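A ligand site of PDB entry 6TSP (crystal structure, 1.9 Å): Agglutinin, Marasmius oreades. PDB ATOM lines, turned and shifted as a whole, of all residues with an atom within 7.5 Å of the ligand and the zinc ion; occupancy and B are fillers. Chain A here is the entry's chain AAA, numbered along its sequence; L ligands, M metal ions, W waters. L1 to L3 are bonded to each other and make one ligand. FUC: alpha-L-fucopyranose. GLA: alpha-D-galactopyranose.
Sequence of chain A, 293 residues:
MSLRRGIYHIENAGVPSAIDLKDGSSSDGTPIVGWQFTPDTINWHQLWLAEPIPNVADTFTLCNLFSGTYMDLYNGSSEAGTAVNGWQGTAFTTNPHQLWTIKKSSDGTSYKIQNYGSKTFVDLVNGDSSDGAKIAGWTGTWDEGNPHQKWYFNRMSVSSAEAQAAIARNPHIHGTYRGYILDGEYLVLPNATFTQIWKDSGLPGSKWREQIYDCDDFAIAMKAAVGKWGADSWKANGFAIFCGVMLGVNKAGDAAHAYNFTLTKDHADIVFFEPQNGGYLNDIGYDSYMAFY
An oxygen (O6) of GLA L2 lies within hydrogen-bond range of a ring nitrogen (ND1) of His 148 (2.9 Å).
O4 of GLA L2 is in hydrogen-bond range of OD2 of Asp 123.
OE2 of Glu 144 lies within hydrogen-bond range of O2 of GLA L3 (2.6 Å).
N of Asn 126 is in hydrogen-bond range of O6 of GLA L2.
The side-chain amide nitrogen (ND2) of Asn 146 is in hydrogen-bond range of an oxygen (O2) of GLA L3, at 2.7 Å.
An oxygen (O4) of GLA L3 sits at hydrogen-bond distance from the side-chain hydroxyl (OG1) of Thr 139, at 2.9 Å.
The indole nitrogen of Trp 138 is in hydrogen-bond range of an oxygen (O5) of GLA L3, at 3.0 Å.
O of His 148 lies within hydrogen-bond range of N of Leu 124 (2.8 Å).
OD1 of Asp 123 lies within hydrogen-bond range of N of Val 125.
O of Ala 136 sits at hydrogen-bond distance from N of Asp 123, 2.8 Å away.
The side-chain carboxylate (OE2) of Glu 144 lies within hydrogen-bond range of the backbone NH (N) of Thr 141 (2.9 Å).
The side-chain carboxylate (OE2) of Glu 144 is in salt-bridge range of the side-chain amino group (NZ) of Lys 112 (3.3 Å).
O of Trp 138 is in hydrogen-bond range of N of Phe 121, at 2.7 Å.
N of Val 125 lies within hydrogen-bond range of O of Lys 134 (3.1 Å).
The side-chain amide oxygen of Gln 149 lies within hydrogen-bond range of the side-chain amino group of Lys 112, at 2.9 Å.
Merely in contact with the ligand: Val 125 (3.3 Å), Leu 124 (3.5 Å), Gln 149 (3.7 Å) and Gly 140 (3.9 Å).
Hydrophobic or aromatic side chains within 4 Å of the ligand: Trp 138 and His 148.
The nearest printed residue that does not touch the ligand is Gly 127 (4.4 Å).
Of the 23 residues printed, 1 comes within 4 Å of the zinc ion.
The nearest printed residue that does not touch the zinc ion is Asn 126 (4.2 Å).
The zinc ion is bound by NE2 of His 148.
Water W4 binds the zinc ion, 2.5 Å away.
Water W1 bridges OD1 of Asn 146 (2.9 Å) and O5 of FUC L1 (2.9 Å).
Water W2 bridges an oxygen (O6) of GLA L3 and the indole nitrogen (NE1) of Trp 138.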
ATOM      1  N   GLY A  14     -11.305  35.669  20.660  1.00  0.00           N
ATOM      2  CA  GLY A  14     -10.540  34.667  21.430  1.00  0.00           C
ATOM      3  C   GLY A  14      -9.052  34.996  21.463  1.00  0.00           C
ATOM      4  O   GLY A  14      -8.432  34.760  22.522  1.00  0.00           O
ATOM      5  N   VAL A  15      -8.483  35.336  20.325  1.00  0.00           N
ATOM      6  CA  VAL A  15      -7.029  35.604  20.208  1.00  0.00           C
ATOM      7  C   VAL A  15      -6.817  36.877  19.392  1.00  0.00           C
ATOM      8  O   VAL A  15      -7.652  37.228  18.578  1.00  0.00           O
ATOM      9  CB  VAL A  15      -6.289  34.399  19.579  1.00  0.00           C
ATOM     10  CG1 VAL A  15      -6.375  33.137  20.455  1.00  0.00           C
ATOM     11  CG2 VAL A  15      -6.788  34.104  18.165  1.00  0.00           C
ATOM     12  N   ALA A  80     -18.506  22.644   6.385  1.00  0.00           N
ATOM     13  CA  ALA A  80     -17.541  23.146   7.386  1.00  0.00           C
ATOM     14  C   ALA A  80     -16.134  23.083   6.801  1.00  0.00           C
ATOM     15  O   ALA A  80     -15.759  22.027   6.277  1.00  0.00           O
ATOM     16  CB  ALA A  80     -17.643  22.340   8.662  1.00  0.00           C
ATOM     17  N   LYS A 112     -21.099  37.983  15.060  1.00  0.00           N
ATOM     18  CA  LYS A 112     -20.898  36.813  14.217  1.00  0.00           C
ATOM     19  C   LYS A 112     -21.200  37.188  12.755  1.00  0.00           C
ATOM     20  O   LYS A 112     -21.980  38.138  12.541  1.00  0.00           O
ATOM     21  CB  LYS A 112     -21.789  35.658  14.696  1.00  0.00           C
ATOM     22  CG  LYS A 112     -21.559  35.211  16.147  1.00  0.00           C
ATOM     23  CD  LYS A 112     -22.064  33.825  16.454  1.00  0.00           C
ATOM     24  CE  LYS A 112     -21.346  32.743  15.666  1.00  0.00           C
ATOM     25  NZ  LYS A 112     -21.390  31.425  16.365  1.00  0.00           N
ATOM     26  N   PHE A 121     -20.881  30.251   9.355  1.00  0.00           N
ATOM     27  CA  PHE A 121     -20.284  31.411  10.044  1.00  0.00           C
ATOM     28  C   PHE A 121     -18.789  31.485   9.704  1.00  0.00           C
ATOM     29  O   PHE A 121     -18.119  30.412   9.638  1.00  0.00           O
ATOM     30  CB  PHE A 121     -20.534  31.326  11.551  1.00  0.00           C
ATOM     31  CG  PHE A 121     -21.972  31.536  11.955  1.00  0.00           C
ATOM     32  CD1 PHE A 121     -22.488  32.825  12.105  1.00  0.00           C
ATOM     33  CD2 PHE A 121     -22.827  30.459  12.164  1.00  0.00           C
ATOM     34  CE1 PHE A 121     -23.810  33.022  12.505  1.00  0.00           C
ATOM     35  CE2 PHE A 121     -24.157  30.663  12.538  1.00  0.00           C
ATOM     36  CZ  PHE A 121     -24.644  31.932  12.719  1.00  0.00           C
ATOM     37  N   ASP A 123     -15.126  31.605  10.655  1.00  0.00           N
ATOM     38  CA  ASP A 123     -14.581  30.814  11.774  1.00  0.00           C
ATOM     39  C   ASP A 123     -13.055  30.773  11.655  1.00  0.00           C
ATOM     40  O   ASP A 123     -12.548  30.393  10.566  1.00  0.00           O
ATOM     41  CB  ASP A 123     -15.209  29.421  11.796  1.00  0.00           C
ATOM     42  CG  ASP A 123     -14.669  28.527  12.896  1.00  0.00           C
ATOM     43  OD1 ASP A 123     -13.433  28.392  12.983  1.00  0.00           O
ATOM     44  OD2 ASP A 123     -15.491  27.966  13.659  1.00  0.00           O
ATOM     45  N   LEU A 124     -12.369  31.253  12.676  1.00  0.00           N
ATOM     46  CA  LEU A 124     -10.905  31.145  12.785  1.00  0.00           C
ATOM     47  C   LEU A 124     -10.562  29.723  13.245  1.00  0.00           C
ATOM     48  O   LEU A 124     -10.845  29.408  14.400  1.00  0.00           O
ATOM     49  CB  LEU A 124     -10.393  32.189  13.765  1.00  0.00           C
ATOM     50  CG  LEU A 124      -8.893  32.173  14.017  1.00  0.00           C
ATOM     51  CD1 LEU A 124      -8.112  32.427  12.721  1.00  0.00           C
ATOM     52  CD2 LEU A 124      -8.520  33.189  15.076  1.00  0.00           C
ATOM     53  N   VAL A 125     -10.241  28.850  12.303  1.00  0.00           N
ATOM     54  CA  VAL A 125     -10.295  27.371  12.514  1.00  0.00           C
ATOM     55  C   VAL A 125      -9.387  27.018  13.704  1.00  0.00           C
ATOM     56  O   VAL A 125      -8.200  27.465  13.703  1.00  0.00           O
ATOM     57  CB  VAL A 125      -9.901  26.608  11.237  1.00  0.00           C
ATOM     58  CG1 VAL A 125      -9.929  25.062  11.451  1.00  0.00           C
ATOM     59  CG2 VAL A 125     -10.783  26.993  10.062  1.00  0.00           C
ATOM     60  N   ASN A 126      -9.982  26.458  14.768  1.00  0.00           N
ATOM     61  CA  ASN A 126      -9.247  25.889  15.935  1.00  0.00           C
ATOM     62  C   ASN A 126      -8.794  27.013  16.857  1.00  0.00           C
ATOM     63  O   ASN A 126      -7.985  26.730  17.768  1.00  0.00           O
ATOM     64  CB  ASN A 126      -8.059  25.047  15.483  1.00  0.00           C
ATOM     65  CG  ASN A 126      -8.425  23.640  15.188  1.00  0.00           C
ATOM     66  OD1 ASN A 126      -9.399  23.118  15.751  1.00  0.00           O
ATOM     67  ND2 ASN A 126      -7.713  23.009  14.270  1.00  0.00           N
ATOM     68  N   GLY A 127      -9.255  28.229  16.597  1.00  0.00           N
ATOM     69  CA  GLY A 127      -8.821  29.426  17.345  1.00  0.00           C
ATOM     70  C   GLY A 127      -7.333  29.624  17.227  1.00  0.00           C
ATOM     71  O   GLY A 127      -6.739  30.139  18.174  1.00  0.00           O
ATOM     72  N   ASP A 128      -6.766  29.252  16.097  1.00  0.00           N
ATOM     73  CA  ASP A 128      -5.311  29.312  15.845  1.00  0.00           C
ATOM     74  C   ASP A 128      -4.886  30.768  15.724  1.00  0.00           C
ATOM     75  O   ASP A 128      -5.319  31.432  14.749  1.00  0.00           O
ATOM     76  CB  ASP A 128      -4.954  28.503  14.599  1.00  0.00           C
ATOM     77  CG  ASP A 128      -3.459  28.255  14.403  1.00  0.00           C
ATOM     78  OD1 ASP A 128      -2.635  28.990  15.030  1.00  0.00           O
ATOM     79  OD2 ASP A 128      -3.131  27.429  13.572  1.00  0.00           O
ATOM     80  N   LYS A 134      -5.917  29.497   8.916  1.00  0.00           N
ATOM     81  CA  LYS A 134      -7.106  29.362   8.052  1.00  0.00           C
ATOM     82  C   LYS A 134      -8.288  30.131   8.676  1.00  0.00           C
ATOM     83  O   LYS A 134      -8.559  29.951   9.924  1.00  0.00           O
ATOM     84  CB  LYS A 134      -7.442  27.881   7.850  1.00  0.00           C
ATOM     85  CG  LYS A 134      -8.533  27.590   6.810  1.00  0.00           C
ATOM     86  CD  LYS A 134      -8.695  26.076   6.493  1.00  0.00           C
ATOM     87  CE  LYS A 134      -9.707  25.799   5.391  1.00  0.00           C
ATOM     88  NZ  LYS A 134     -10.045  24.345   5.305  1.00  0.00           N
ATOM     89  N   ALA A 136     -12.471  30.021   7.729  1.00  0.00           N
ATOM     90  CA  ALA A 136     -13.380  29.173   6.938  1.00  0.00           C
ATOM     91  C   ALA A 136     -14.827  29.474   7.294  1.00  0.00           C
ATOM     92  O   ALA A 136     -15.073  29.857   8.448  1.00  0.00           O
ATOM     93  CB  ALA A 136     -13.051  27.715   7.186  1.00  0.00           C
ATOM     94  N   TRP A 138     -18.169  27.816   8.602  1.00  0.00           N
ATOM     95  CA  TRP A 138     -18.322  26.688   9.568  1.00  0.00           C
ATOM     96  C   TRP A 138     -19.746  26.680  10.124  1.00  0.00           C
ATOM     97  O   TRP A 138     -20.336  27.767  10.260  1.00  0.00           O
ATOM     98  CB  TRP A 138     -17.273  26.801  10.681  1.00  0.00           C
ATOM     99  CG  TRP A 138     -16.865  25.481  11.255  1.00  0.00           C
ATOM    100  CD1 TRP A 138     -17.595  24.680  12.076  1.00  0.00           C
ATOM    101  CD2 TRP A 138     -15.642  24.772  10.997  1.00  0.00           C
ATOM    102  NE1 TRP A 138     -16.908  23.540  12.371  1.00  0.00           N
ATOM    103  CE2 TRP A 138     -15.692  23.579  11.740  1.00  0.00           C
ATOM    104  CE3 TRP A 138     -14.507  25.035  10.223  1.00  0.00           C
ATOM    105  CZ2 TRP A 138     -14.666  22.635  11.710  1.00  0.00           C
ATOM    106  CZ3 TRP A 138     -13.489  24.113  10.201  1.00  0.00           C
ATOM    107  CH2 TRP A 138     -13.567  22.920  10.939  1.00  0.00           C
ATOM    108  N   THR A 139     -20.308  25.492  10.342  1.00  0.00           N
ATOM    109  CA  THR A 139     -21.553  25.313  11.100  1.00  0.00           C
ATOM    110  C   THR A 139     -21.459  26.102  12.393  1.00  0.00           C
ATOM    111  O   THR A 139     -20.374  26.170  12.950  1.00  0.00           O
ATOM    112  CB  THR A 139     -21.822  23.827  11.367  1.00  0.00           C
ATOM    113  OG1 THR A 139     -20.680  23.283  12.039  1.00  0.00           O
ATOM    114  CG2 THR A 139     -22.089  23.042  10.103  1.00  0.00           C
ATOM    115  N   GLY A 140     -22.567  26.646  12.845  1.00  0.00           N
ATOM    116  CA  GLY A 140     -22.698  27.144  14.222  1.00  0.00           C
ATOM    117  C   GLY A 140     -24.006  27.833  14.435  1.00  0.00           C
ATOM    118  O   GLY A 140     -24.896  27.700  13.562  1.00  0.00           O
ATOM    119  N   THR A 141     -24.175  28.459  15.589  1.00  0.00           N
ATOM    120  CA  THR A 141     -25.445  29.115  15.965  1.00  0.00           C
ATOM    121  C   THR A 141     -25.190  30.597  16.280  1.00  0.00           C
ATOM    122  O   THR A 141     -24.034  30.930  16.699  1.00  0.00           O
ATOM    123  CB  THR A 141     -26.106  28.397  17.155  1.00  0.00           C
ATOM    124  OG1 THR A 141     -25.309  28.644  18.315  1.00  0.00           O
ATOM    125  CG2 THR A 141     -26.266  26.910  16.937  1.00  0.00           C
ATOM    126  N   GLU A 144     -24.335  30.851  20.564  1.00  0.00           N
ATOM    127  CA  GLU A 144     -23.260  30.078  21.289  1.00  0.00           C
ATOM    128  C   GLU A 144     -22.046  30.987  21.590  1.00  0.00           C
ATOM    129  O   GLU A 144     -21.853  31.951  20.867  1.00  0.00           O
ATOM    130  CB  GLU A 144     -22.852  28.838  20.488  1.00  0.00           C
ATOM    131  CG  GLU A 144     -22.191  29.184  19.150  1.00  0.00           C
ATOM    132  CD  GLU A 144     -21.925  27.985  18.269  1.00  0.00           C
ATOM    133  OE1 GLU A 144     -21.932  26.828  18.807  1.00  0.00           O
ATOM    134  OE2 GLU A 144     -21.695  28.177  17.077  1.00  0.00           O
ATOM    135  N   GLY A 145     -21.233  30.622  22.578  1.00  0.00           N
ATOM    136  CA  GLY A 145     -20.110  31.451  23.066  1.00  0.00           C
ATOM    137  C   GLY A 145     -18.853  31.272  22.214  1.00  0.00           C
ATOM    138  O   GLY A 145     -17.932  32.052  22.380  1.00  0.00           O
ATOM    139  N   ASN A 146     -18.820  30.211  21.389  1.00  0.00           N
ATOM    140  CA  ASN A 146     -17.636  29.773  20.616  1.00  0.00           C
ATOM    141  C   ASN A 146     -16.876  30.994  20.077  1.00  0.00           C
ATOM    142  O   ASN A 146     -17.356  31.673  19.191  1.00  0.00           O
ATOM    143  CB  ASN A 146     -18.037  28.828  19.493  1.00  0.00           C
ATOM    144  CG  ASN A 146     -16.873  28.401  18.615  1.00  0.00           C
ATOM    145  OD1 ASN A 146     -15.727  28.723  18.902  1.00  0.00           O
ATOM    146  ND2 ASN A 146     -17.165  27.668  17.543  1.00  0.00           N
ATOM    147  N   PRO A 147     -15.665  31.302  20.609  1.00  0.00           N
ATOM    148  CA  PRO A 147     -14.959  32.538  20.224  1.00  0.00           C
ATOM    149  C   PRO A 147     -14.249  32.410  18.849  1.00  0.00           C
ATOM    150  O   PRO A 147     -13.874  33.478  18.269  1.00  0.00           O
ATOM    151  CB  PRO A 147     -13.916  32.762  21.347  1.00  0.00           C
ATOM    152  CG  PRO A 147     -13.761  31.374  22.020  1.00  0.00           C
ATOM    153  CD  PRO A 147     -15.088  30.662  21.796  1.00  0.00           C
ATOM    154  N   HIS A 148     -14.182  31.211  18.299  1.00  0.00           N
ATOM    155  CA  HIS A 148     -13.671  30.996  16.930  1.00  0.00           C
ATOM    156  C   HIS A 148     -14.511  31.808  15.950  1.00  0.00           C
ATOM    157  O   HIS A 148     -14.033  32.028  14.818  1.00  0.00           O
ATOM    158  CB  HIS A 148     -13.677  29.515  16.560  1.00  0.00           C
ATOM    159  CG  HIS A 148     -12.847  28.657  17.447  1.00  0.00           C
ATOM    160  ND1 HIS A 148     -12.796  27.293  17.306  1.00  0.00           N
ATOM    161  CD2 HIS A 148     -12.117  28.939  18.554  1.00  0.00           C
ATOM    162  CE1 HIS A 148     -12.101  26.776  18.285  1.00  0.00           C
ATOM    163  NE2 HIS A 148     -11.652  27.773  19.042  1.00  0.00           N
ATOM    164  N   GLN A 149     -15.795  32.045  16.278  1.00  0.00           N
ATOM    165  CA  GLN A 149     -16.792  32.602  15.328  1.00  0.00           C
ATOM    166  C   GLN A 149     -17.280  33.976  15.839  1.00  0.00           C
ATOM    167  O   GLN A 149     -18.190  34.517  15.233  1.00  0.00           O
ATOM    168  CB  GLN A 149     -17.955  31.629  15.154  1.00  0.00           C
ATOM    169  CG  GLN A 149     -17.533  30.272  14.617  1.00  0.00           C
ATOM    170  CD  GLN A 149     -18.713  29.376  14.293  1.00  0.00           C
ATOM    171  OE1 GLN A 149     -19.857  29.750  14.518  1.00  0.00           O
ATOM    172  NE2 GLN A 149     -18.429  28.214  13.709  1.00  0.00           N
HETATM  173  C1  FUC L   1     -16.911  23.850  19.675  1.00  0.00           C
HETATM  174  C2  FUC L   1     -17.670  22.672  20.318  1.00  0.00           C
HETATM  175  C3  FUC L   1     -16.733  21.587  20.875  1.00  0.00           C
HETATM  176  C4  FUC L   1     -15.609  22.190  21.649  1.00  0.00           C
HETATM  177  C5  FUC L   1     -14.884  23.244  20.806  1.00  0.00           C
HETATM  178  C6  FUC L   1     -13.678  23.817  21.527  1.00  0.00           C
HETATM  179  O2  FUC L   1     -18.517  22.053  19.361  1.00  0.00           O
HETATM  180  O3  FUC L   1     -17.471  20.698  21.729  1.00  0.00           O
HETATM  181  O4  FUC L   1     -16.141  22.785  22.842  1.00  0.00           O
HETATM  182  O5  FUC L   1     -15.810  24.298  20.507  1.00  0.00           O
HETATM  183  C1  GLA L   2     -13.997  23.693  17.388  1.00  0.00           C
HETATM  184  C2  GLA L   2     -15.376  24.283  17.621  1.00  0.00           C
HETATM  185  C3  GLA L   2     -16.172  24.234  16.337  1.00  0.00           C
HETATM  186  C4  GLA L   2     -15.427  25.018  15.267  1.00  0.00           C
HETATM  187  C5  GLA L   2     -14.027  24.429  15.074  1.00  0.00           C
HETATM  188  C6  GLA L   2     -13.236  25.193  13.990  1.00  0.00           C
HETATM  189  O1  GLA L   2     -14.126  22.294  17.029  1.00  0.00           O
HETATM  190  O2  GLA L   2     -16.066  23.536  18.635  1.00  0.00           O
HETATM  191  O3  GLA L   2     -17.488  24.788  16.539  1.00  0.00           O
HETATM  192  O4  GLA L   2     -15.370  26.419  15.629  1.00  0.00           O
HETATM  193  O5  GLA L   2     -13.301  24.430  16.346  1.00  0.00           O
HETATM  194  O6  GLA L   2     -12.683  26.399  14.514  1.00  0.00           O
HETATM  195  C1  GLA L   3     -18.413  25.001  15.625  1.00  0.00           C
HETATM  196  C2  GLA L   3     -19.749  25.427  16.085  1.00  0.00           C
HETATM  197  C3  GLA L   3     -20.447  24.286  16.856  1.00  0.00           C
HETATM  198  C4  GLA L   3     -20.416  23.012  16.020  1.00  0.00           C
HETATM  199  C5  GLA L   3     -18.998  22.710  15.559  1.00  0.00           C
HETATM  200  C6  GLA L   3     -18.916  21.475  14.654  1.00  0.00           C
HETATM  201  O2  GLA L   3     -19.602  26.567  16.954  1.00  0.00           O
HETATM  202  O3  GLA L   3     -21.790  24.675  17.169  1.00  0.00           O
HETATM  203  O4  GLA L   3     -21.266  23.144  14.874  1.00  0.00           O
HETATM  204  O5  GLA L   3     -18.513  23.828  14.839  1.00  0.00           O
HETATM  205  O6  GLA L   3     -17.533  21.122  14.430  1.00  0.00           O
HETATM  206 ZN    ZN M   1     -10.655  27.424  20.882  1.00  0.00          ZN
HETATM  207  O   HOH W   1     -14.724  26.955  20.980  1.00  0.00           O
HETATM  208  O   HOH W   2     -17.080  20.364  11.582  1.00  0.00           O
HETATM  209  O   HOH W   3     -11.817  25.603  22.840  1.00  0.00           O
HETATM  210  O   HOH W   4     -10.418  29.253  22.572  1.00  0.00           O
